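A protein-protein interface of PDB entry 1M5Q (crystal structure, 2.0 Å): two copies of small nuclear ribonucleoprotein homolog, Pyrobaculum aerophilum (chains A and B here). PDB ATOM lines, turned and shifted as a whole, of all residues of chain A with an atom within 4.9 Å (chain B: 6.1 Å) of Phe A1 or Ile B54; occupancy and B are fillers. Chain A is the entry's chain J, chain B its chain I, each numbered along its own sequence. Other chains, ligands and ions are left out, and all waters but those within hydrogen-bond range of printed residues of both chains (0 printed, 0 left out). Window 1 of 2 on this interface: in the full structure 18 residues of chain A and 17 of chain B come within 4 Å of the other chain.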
ATOM      1  N   PHE A   1     -12.834  10.081 -30.098  1.00  0.00           N
ATOM      2  CA  PHE A   1     -13.024  11.546 -29.933  1.00  0.00           C
ATOM      3  C   PHE A   1     -11.709  12.289 -29.970  1.00  0.00           C
ATOM      4  O   PHE A   1     -11.488  13.244 -29.220  1.00  0.00           O
ATOM      5  CB  PHE A   1     -13.777  11.848 -28.615  1.00  0.00           C
ATOM      6  CG  PHE A   1     -13.511  10.833 -27.534  1.00  0.00           C
ATOM      7  CD1 PHE A   1     -14.469   9.889 -27.206  1.00  0.00           C
ATOM      8  CD2 PHE A   1     -12.267  10.790 -26.906  1.00  0.00           C
ATOM      9  CE1 PHE A   1     -14.183   8.887 -26.246  1.00  0.00           C
ATOM     10  CE2 PHE A   1     -11.958   9.806 -25.952  1.00  0.00           C
ATOM     11  CZ  PHE A   1     -12.919   8.850 -25.624  1.00  0.00           C
ATOM     12  N   VAL A   2     -10.838  11.836 -30.853  1.00  0.00           N
ATOM     13  CA  VAL A   2      -9.559  12.458 -31.069  1.00  0.00           C
ATOM     14  C   VAL A   2      -9.779  13.940 -31.458  1.00  0.00           C
ATOM     15  O   VAL A   2      -9.101  14.840 -30.960  1.00  0.00           O
ATOM     16  CB  VAL A   2      -8.824  11.739 -32.255  1.00  0.00           C
ATOM     17  CG1 VAL A   2      -7.620  12.579 -32.738  1.00  0.00           C
ATOM     18  CG2 VAL A   2      -8.388  10.369 -31.819  1.00  0.00           C
ATOM     19  N   ALA A   3     -10.718  14.195 -32.361  1.00  0.00           N
ATOM     20  CA  ALA A   3     -10.946  15.583 -32.788  1.00  0.00           C
ATOM     21  C   ALA A   3     -11.456  16.463 -31.629  1.00  0.00           C
ATOM     22  O   ALA A   3     -10.956  17.590 -31.426  1.00  0.00           O
ATOM     23  CB  ALA A   3     -11.927  15.632 -33.947  1.00  0.00           C
ATOM     24  N   GLU A   4     -12.435  15.965 -30.878  1.00  0.00           N
ATOM     25  CA  GLU A   4     -12.956  16.743 -29.761  1.00  0.00           C
ATOM     26  C   GLU A   4     -11.834  17.084 -28.757  1.00  0.00           C
ATOM     27  O   GLU A   4     -11.755  18.228 -28.270  1.00  0.00           O
ATOM     28  CB  GLU A   4     -14.139  16.015 -29.046  1.00  0.00           C
ATOM     29  CG  GLU A   4     -15.513  16.184 -29.748  1.00  0.00           C
ATOM     30  CD  GLU A   4     -16.758  16.287 -28.791  1.00  0.00           C
ATOM     31  OE1 GLU A   4     -16.852  17.214 -27.939  1.00  0.00           O
ATOM     32  OE2 GLU A   4     -17.683  15.441 -28.901  1.00  0.00           O
ATOM     33  N   LEU A   5     -10.954  16.127 -28.452  1.00  0.00           N
ATOM     34  CA  LEU A   5      -9.856  16.404 -27.493  1.00  0.00           C
ATOM     35  C   LEU A   5      -8.762  17.297 -28.064  1.00  0.00           C
ATOM     36  O   LEU A   5      -8.131  18.067 -27.344  1.00  0.00           O
ATOM     37  CB  LEU A   5      -9.222  15.095 -26.981  1.00  0.00           C
ATOM     38  CG  LEU A   5     -10.115  14.180 -26.145  1.00  0.00           C
ATOM     39  CD1 LEU A   5      -9.363  12.958 -25.687  1.00  0.00           C
ATOM     40  CD2 LEU A   5     -10.591  14.948 -24.952  1.00  0.00           C
ATOM     41  N   LEU A  34      -5.341   7.796 -29.034  1.00  0.00           N
ATOM     42  CA  LEU A  34      -5.866   8.297 -27.776  1.00  0.00           C
ATOM     43  C   LEU A  34      -4.837   8.170 -26.604  1.00  0.00           C
ATOM     44  O   LEU A  34      -5.200   8.091 -25.439  1.00  0.00           O
ATOM     45  CB  LEU A  34      -7.217   7.613 -27.494  1.00  0.00           C
ATOM     46  CG  LEU A  34      -8.565   8.351 -27.723  1.00  0.00           C
ATOM     47  CD1 LEU A  34      -8.396   9.663 -28.447  1.00  0.00           C
ATOM     48  CD2 LEU A  34      -9.569   7.480 -28.425  1.00  0.00           C
ATOM     49  N   VAL A  60      -9.577   5.050 -18.657  1.00  0.00           N
ATOM     50  CA  VAL A  60     -10.996   4.703 -18.579  1.00  0.00           C
ATOM     51  C   VAL A  60     -11.826   5.838 -19.237  1.00  0.00           C
ATOM     52  O   VAL A  60     -12.644   5.623 -20.150  1.00  0.00           O
ATOM     53  CB  VAL A  60     -11.387   4.438 -17.090  1.00  0.00           C
ATOM     54  CG1 VAL A  60     -12.791   3.907 -17.003  1.00  0.00           C
ATOM     55  CG2 VAL A  60     -10.402   3.433 -16.478  1.00  0.00           C
ATOM     56  N   HIS A  61     -11.570   7.069 -18.822  1.00  0.00           N
ATOM     57  CA  HIS A  61     -12.250   8.209 -19.406  1.00  0.00           C
ATOM     58  C   HIS A  61     -11.478   9.505 -19.167  1.00  0.00           C
ATOM     59  O   HIS A  61     -10.582   9.575 -18.286  1.00  0.00           O
ATOM     60  CB  HIS A  61     -13.699   8.339 -18.866  1.00  0.00           C
ATOM     61  CG  HIS A  61     -13.815   8.553 -17.373  1.00  0.00           C
ATOM     62  ND1 HIS A  61     -13.910   7.516 -16.466  1.00  0.00           N
ATOM     63  CD2 HIS A  61     -13.886   9.687 -16.641  1.00  0.00           C
ATOM     64  CE1 HIS A  61     -14.042   7.999 -15.244  1.00  0.00           C
ATOM     65  NE2 HIS A  61     -14.032   9.315 -15.324  1.00  0.00           N
ATOM     66  N   ILE A  62     -11.822  10.521 -19.958  1.00  0.00           N
ATOM     67  CA  ILE A  62     -11.198  11.850 -19.823  1.00  0.00           C
ATOM     68  C   ILE A  62     -12.351  12.818 -19.532  1.00  0.00           C
ATOM     69  O   ILE A  62     -13.350  12.793 -20.207  1.00  0.00           O
ATOM     70  CB  ILE A  62     -10.536  12.399 -21.133  1.00  0.00           C
ATOM     71  CG1 ILE A  62      -9.760  11.315 -21.895  1.00  0.00           C
ATOM     72  CG2 ILE A  62      -9.675  13.568 -20.785  1.00  0.00           C
ATOM     73  CD1 ILE A  62      -8.843  10.526 -21.100  1.00  0.00           C
ATOM     74  N   VAL B  15     -23.978   4.833 -18.190  1.00  0.00           N
ATOM     75  CA  VAL B  15     -22.895   4.039 -18.715  1.00  0.00           C
ATOM     76  C   VAL B  15     -22.116   3.466 -17.522  1.00  0.00           C
ATOM     77  O   VAL B  15     -21.533   4.208 -16.714  1.00  0.00           O
ATOM     78  CB  VAL B  15     -21.973   4.890 -19.614  1.00  0.00           C
ATOM     79  CG1 VAL B  15     -20.872   4.007 -20.265  1.00  0.00           C
ATOM     80  CG2 VAL B  15     -22.800   5.592 -20.694  1.00  0.00           C
ATOM     81  N   LEU B  17     -18.964   1.394 -16.146  1.00  0.00           N
ATOM     82  CA  LEU B  17     -17.593   1.137 -16.541  1.00  0.00           C
ATOM     83  C   LEU B  17     -16.987   0.013 -15.703  1.00  0.00           C
ATOM     84  O   LEU B  17     -17.453  -0.277 -14.597  1.00  0.00           O
ATOM     85  CB  LEU B  17     -16.781   2.404 -16.376  1.00  0.00           C
ATOM     86  CG  LEU B  17     -17.424   3.651 -16.972  1.00  0.00           C
ATOM     87  CD1 LEU B  17     -16.438   4.819 -16.765  1.00  0.00           C
ATOM     88  CD2 LEU B  17     -17.773   3.472 -18.445  1.00  0.00           C
ATOM     89  N   TYR B  23     -21.552   6.466 -14.828  1.00  0.00           N
ATOM     90  CA  TYR B  23     -21.850   7.848 -15.225  1.00  0.00           C
ATOM     91  C   TYR B  23     -23.260   7.997 -15.842  1.00  0.00           C
ATOM     92  O   TYR B  23     -23.714   7.161 -16.642  1.00  0.00           O
ATOM     93  CB  TYR B  23     -20.807   8.381 -16.230  1.00  0.00           C
ATOM     94  CG  TYR B  23     -19.532   8.764 -15.579  1.00  0.00           C
ATOM     95  CD1 TYR B  23     -19.305  10.095 -15.166  1.00  0.00           C
ATOM     96  CD2 TYR B  23     -18.603   7.787 -15.215  1.00  0.00           C
ATOM     97  CE1 TYR B  23     -18.170  10.440 -14.374  1.00  0.00           C
ATOM     98  CE2 TYR B  23     -17.460   8.115 -14.421  1.00  0.00           C
ATOM     99  CZ  TYR B  23     -17.261   9.428 -14.000  1.00  0.00           C
ATOM    100  OH  TYR B  23     -16.214   9.702 -13.143  1.00  0.00           O
ATOM    101  N   ASP B  31     -19.321   6.647 -31.493  1.00  0.00           N
ATOM    102  CA  ASP B  31     -18.676   6.442 -32.786  1.00  0.00           C
ATOM    103  C   ASP B  31     -18.770   4.938 -33.125  1.00  0.00           C
ATOM    104  O   ASP B  31     -19.325   4.174 -32.337  1.00  0.00           O
ATOM    105  CB  ASP B  31     -17.224   7.010 -32.778  1.00  0.00           C
ATOM    106  CG  ASP B  31     -16.313   6.336 -31.777  1.00  0.00           C
ATOM    107  OD1 ASP B  31     -15.219   6.898 -31.536  1.00  0.00           O
ATOM    108  OD2 ASP B  31     -16.657   5.241 -31.247  1.00  0.00           O
ATOM    109  N   LEU B  34     -17.826   2.432 -30.579  1.00  0.00           N
ATOM    110  CA  LEU B  34     -18.614   2.584 -29.340  1.00  0.00           C
ATOM    111  C   LEU B  34     -17.913   3.409 -28.234  1.00  0.00           C
ATOM    112  O   LEU B  34     -18.069   3.114 -27.041  1.00  0.00           O
ATOM    113  CB  LEU B  34     -19.063   1.228 -28.796  1.00  0.00           C
ATOM    114  CG  LEU B  34     -20.434   0.633 -29.168  1.00  0.00           C
ATOM    115  CD1 LEU B  34     -21.246   1.546 -30.098  1.00  0.00           C
ATOM    116  CD2 LEU B  34     -20.266  -0.802 -29.716  1.00  0.00           C
ATOM    117  N   ASN B  35     -17.069   4.372 -28.650  1.00  0.00           N
ATOM    118  CA  ASN B  35     -16.492   5.340 -27.714  1.00  0.00           C
ATOM    119  C   ASN B  35     -17.740   6.200 -27.480  1.00  0.00           C
ATOM    120  O   ASN B  35     -18.590   6.289 -28.343  1.00  0.00           O
ATOM    121  CB  ASN B  35     -15.379   6.174 -28.337  1.00  0.00           C
ATOM    122  CG  ASN B  35     -14.073   5.428 -28.421  1.00  0.00           C
ATOM    123  OD1 ASN B  35     -13.620   4.791 -27.449  1.00  0.00           O
ATOM    124  ND2 ASN B  35     -13.450   5.502 -29.575  1.00  0.00           N
ATOM    125  N   ILE B  36     -17.850   6.812 -26.315  1.00  0.00           N
ATOM    126  CA  ILE B  36     -19.061   7.540 -25.915  1.00  0.00           C
ATOM    127  C   ILE B  36     -18.702   8.853 -25.267  1.00  0.00           C
ATOM    128  O   ILE B  36     -17.826   8.889 -24.432  1.00  0.00           O
ATOM    129  CB  ILE B  36     -19.816   6.757 -24.811  1.00  0.00           C
ATOM    130  CG1 ILE B  36     -20.186   5.363 -25.312  1.00  0.00           C
ATOM    131  CG2 ILE B  36     -21.051   7.572 -24.318  1.00  0.00           C
ATOM    132  CD1 ILE B  36     -21.381   5.304 -26.156  1.00  0.00           C
ATOM    133  N   VAL B  37     -19.382   9.921 -25.662  1.00  0.00           N
ATOM    134  CA  VAL B  37     -19.196  11.204 -25.035  1.00  0.00           C
ATOM    135  C   VAL B  37     -20.540  11.504 -24.354  1.00  0.00           C
ATOM    136  O   VAL B  37     -21.574  11.437 -24.992  1.00  0.00           O
ATOM    137  CB  VAL B  37     -18.887  12.353 -26.039  1.00  0.00           C
ATOM    138  CG1 VAL B  37     -18.680  13.691 -25.271  1.00  0.00           C
ATOM    139  CG2 VAL B  37     -17.583  12.072 -26.807  1.00  0.00           C
ATOM    140  N   LEU B  38     -20.504  11.775 -23.051  1.00  0.00           N
ATOM    141  CA  LEU B  38     -21.686  12.189 -22.314  1.00  0.00           C
ATOM    142  C   LEU B  38     -21.534  13.694 -22.021  1.00  0.00           C
ATOM    143  O   LEU B  38     -20.423  14.191 -21.826  1.00  0.00           O
ATOM    144  CB  LEU B  38     -21.820  11.469 -20.972  1.00  0.00           C
ATOM    145  CG  LEU B  38     -21.976   9.972 -21.054  1.00  0.00           C
ATOM    146  CD1 LEU B  38     -22.234   9.460 -19.616  1.00  0.00           C
ATOM    147  CD2 LEU B  38     -23.171   9.615 -21.990  1.00  0.00           C
ATOM    148  N   VAL B  52     -17.753  14.125 -20.579  1.00  0.00           N
ATOM    149  CA  VAL B  52     -16.983  12.965 -20.212  1.00  0.00           C
ATOM    150  C   VAL B  52     -16.726  12.106 -21.490  1.00  0.00           C
ATOM    151  O   VAL B  52     -17.647  11.703 -22.179  1.00  0.00           O
ATOM    152  CB  VAL B  52     -17.694  12.144 -19.149  1.00  0.00           C
ATOM    153  CG1 VAL B  52     -16.909  10.935 -18.852  1.00  0.00           C
ATOM    154  CG2 VAL B  52     -17.858  13.004 -17.873  1.00  0.00           C
ATOM    155  N   PHE B  53     -15.457  11.840 -21.783  1.00  0.00           N
ATOM    156  CA  PHE B  53     -15.090  11.053 -22.961  1.00  0.00           C
ATOM    157  C   PHE B  53     -14.751   9.665 -22.455  1.00  0.00           C
ATOM    158  O   PHE B  53     -13.679   9.451 -21.883  1.00  0.00           O
ATOM    159  CB  PHE B  53     -13.893  11.707 -23.643  1.00  0.00           C
ATOM    160  CG  PHE B  53     -14.167  13.124 -24.089  1.00  0.00           C
ATOM    161  CD1 PHE B  53     -13.955  14.210 -23.226  1.00  0.00           C
ATOM    162  CD2 PHE B  53     -14.618  13.368 -25.390  1.00  0.00           C
ATOM    163  CE1 PHE B  53     -14.182  15.534 -23.667  1.00  0.00           C
ATOM    164  CE2 PHE B  53     -14.848  14.698 -25.838  1.00  0.00           C
ATOM    165  CZ  PHE B  53     -14.626  15.770 -24.975  1.00  0.00           C
ATOM    166  N   ILE B  54     -15.646   8.714 -22.709  1.00  0.00           N
ATOM    167  CA  ILE B  54     -15.453   7.359 -22.187  1.00  0.00           C
ATOM    168  C   ILE B  54     -14.842   6.402 -23.230  1.00  0.00           C
ATOM    169  O   ILE B  54     -15.408   6.268 -24.361  1.00  0.00           O
ATOM    170  CB  ILE B  54     -16.789   6.797 -21.736  1.00  0.00           C
ATOM    171  CG1 ILE B  54     -17.392   7.722 -20.689  1.00  0.00           C
ATOM    172  CG2 ILE B  54     -16.585   5.370 -21.208  1.00  0.00           C
ATOM    173  CD1 ILE B  54     -18.876   7.362 -20.351  1.00  0.00           C
ATOM    174  N   MET B  55     -13.720   5.765 -22.841  1.00  0.00           N
ATOM    175  CA  MET B  55     -12.972   4.833 -23.723  1.00  0.00           C
ATOM    176  C   MET B  55     -13.760   3.530 -23.859  1.00  0.00           C
ATOM    177  O   MET B  55     -14.056   2.860 -22.871  1.00  0.00           O
ATOM    178  CB  MET B  55     -11.581   4.560 -23.151  1.00  0.00           C
ATOM    179  CG  MET B  55     -10.744   5.819 -23.004  1.00  0.00           C
ATOM    180  SD  MET B  55     -10.154   6.616 -24.716  1.00  0.00           S
ATOM    181  CE  MET B  55      -8.493   5.534 -24.837  1.00  0.00           C
ATOM    182  N   TYR B  56     -14.071   3.161 -25.095  1.00  0.00           N
ATOM    183  CA  TYR B  56     -14.901   1.979 -25.331  1.00  0.00           C
ATOM    184  C   TYR B  56     -14.481   0.676 -24.623  1.00  0.00           C
ATOM    185  O   TYR B  56     -15.320  -0.152 -24.244  1.00  0.00           O
ATOM    186  CB  TYR B  56     -15.032   1.758 -26.851  1.00  0.00           C
ATOM    187  CG  TYR B  56     -13.887   0.950 -27.486  1.00  0.00           C
ATOM    188  CD1 TYR B  56     -13.761  -0.423 -27.242  1.00  0.00           C
ATOM    189  CD2 TYR B  56     -12.940   1.574 -28.309  1.00  0.00           C
ATOM    190  CE1 TYR B  56     -12.728  -1.153 -27.798  1.00  0.00           C
ATOM    191  CE2 TYR B  56     -11.898   0.867 -28.888  1.00  0.00           C
ATOM    192  CZ  TYR B  56     -11.796  -0.502 -28.623  1.00  0.00           C
ATOM    193  OH  TYR B  56     -10.751  -1.212 -29.128  1.00  0.00           O
ATOM    194  N   TYR B  58     -13.504   0.098 -21.680  1.00  0.00           N
ATOM    195  CA  TYR B  58     -13.915   0.041 -20.270  1.00  0.00           C
ATOM    196  C   TYR B  58     -15.439   0.123 -20.033  1.00  0.00           C
ATOM    197  O   TYR B  58     -15.913   0.163 -18.884  1.00  0.00           O
ATOM    198  CB  TYR B  58     -13.186   1.161 -19.512  1.00  0.00           C
ATOM    199  CG  TYR B  58     -11.693   0.876 -19.361  1.00  0.00           C
ATOM    200  CD1 TYR B  58     -10.767   1.275 -20.341  1.00  0.00           C
ATOM    201  CD2 TYR B  58     -11.224   0.127 -18.282  1.00  0.00           C
ATOM    202  CE1 TYR B  58      -9.375   0.927 -20.223  1.00  0.00           C
ATOM    203  CE2 TYR B  58      -9.883  -0.242 -18.172  1.00  0.00           C
ATOM    204  CZ  TYR B  58      -8.964   0.169 -19.151  1.00  0.00           C
ATOM    205  OH  TYR B  58      -7.663  -0.226 -19.015  1.00  0.00           O
ATOM    206  N   ILE B  59     -16.195   0.121 -21.127  1.00  0.00           N
ATOM    207  CA  ILE B  59     -17.639   0.181 -21.038  1.00  0.00           C
ATOM    208  C   ILE B  59     -18.202  -1.219 -20.925  1.00  0.00           C
ATOM    209  O   ILE B  59     -18.042  -2.044 -21.838  1.00  0.00           O
ATOM    210  CB  ILE B  59     -18.248   0.855 -22.273  1.00  0.00           C
ATOM    211  CG1 ILE B  59     -17.741   2.290 -22.363  1.00  0.00           C
ATOM    212  CG2 ILE B  59     -19.821   0.799 -22.219  1.00  0.00           C
ATOM    213  CD1 ILE B  59     -18.372   3.079 -23.541  1.00  0.00           C
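The backbone NH (N) of Val B15 lies within hydrogen-bond range of the backbone carbonyl oxygen (O) of Tyr B23, 2.8 Å away.
OD2 of Asp B31 lies within hydrogen-bond range of N of Asn B35 (2.8 Å).
N of Tyr B56 lies within hydrogen-bond range of OD1 of Asn B35 (2.9 Å).
The backbone NH (N) of Ile B54 sits at hydrogen-bond distance from the backbone carbonyl oxygen (O) of Ile B36 (2.8 Å).
The backbone carbonyl oxygen (O) of Leu B38 sits at hydrogen-bond distance from the backbone NH (N) of Val B52.
Phe A1 touches just these residues of chain B: Asn B35 (3.6 Å), Val B37 (3.8 Å), Phe B53 (3.5 Å), Ile B54 (3.5 Å) and Met B55 (3.7 Å).
Ile B54 touches just these residues of chain A: Phe A1 (3.5 Å), Val A60 (3.9 Å) and His A61 (3.9 Å).
Printed residues of chain A within 4 Å of Val B37: Phe A1 (3.8 Å) and Glu A4 (3.97 Å).
Of the printed residues of chain A, Tyr B23 touches His A61.
Of the printed residues of chain B, Glu A4 touches Val B37 (3.97 Å) and Phe B53 (3.5 Å).
Asp B31 touches none of the printed residues of chain A.
NE2 of His A61 sits at hydrogen-bond distance from OH of Tyr B23, 3.1 Å away.
The backbone NH (N) of Phe B53 sits at hydrogen-bond distance from the backbone carbonyl oxygen (O) of Ile A62 (2.8 Å).
N of Met B55 is in hydrogen-bond range of O of Val A60 (2.9 Å).
Position printed for both chains: 34.
CG of Phe A1 touches CD2 of Phe B53, 3.5 Å away.
Ile B54 touches Phe A1.
Met B55 touches Phe A1 (SD to CZ, 3.7 Å).
Glu A4 touches Val B37 (OE2 to CG2, 3.97 Å).
CD1 of Phe B53 touches CD2 of Leu A5, at 3.9 Å.
CD1 of Leu B17 touches CG1 of Val A60, 3.8 Å away.
CG1 of Val A60 touches CB of Tyr B58 (3.7 Å).
ND1 of His A61 touches CD1 of Leu B17 (3.7 Å).
His A61 touches Ile B54 (CB to CA, 3.9 Å).
Val B52 touches Ile A62 (CA to O, 3.6 Å).
Printed residues of chain A that touch a printed residue of chain B: Phe A1, Glu A4, Leu A5, Leu A34, Val A60, His A61 and Ile A62.
Hydrophobic or aromatic side chains of chain A that line the printed part of chain B: Phe A1, Leu A5, Leu A34, Val A60 and His A61.
Of the 16 printed residues of chain B, 9 touch a printed residue of chain A.
Among the printed residues, 20 pairs touch across the chains.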
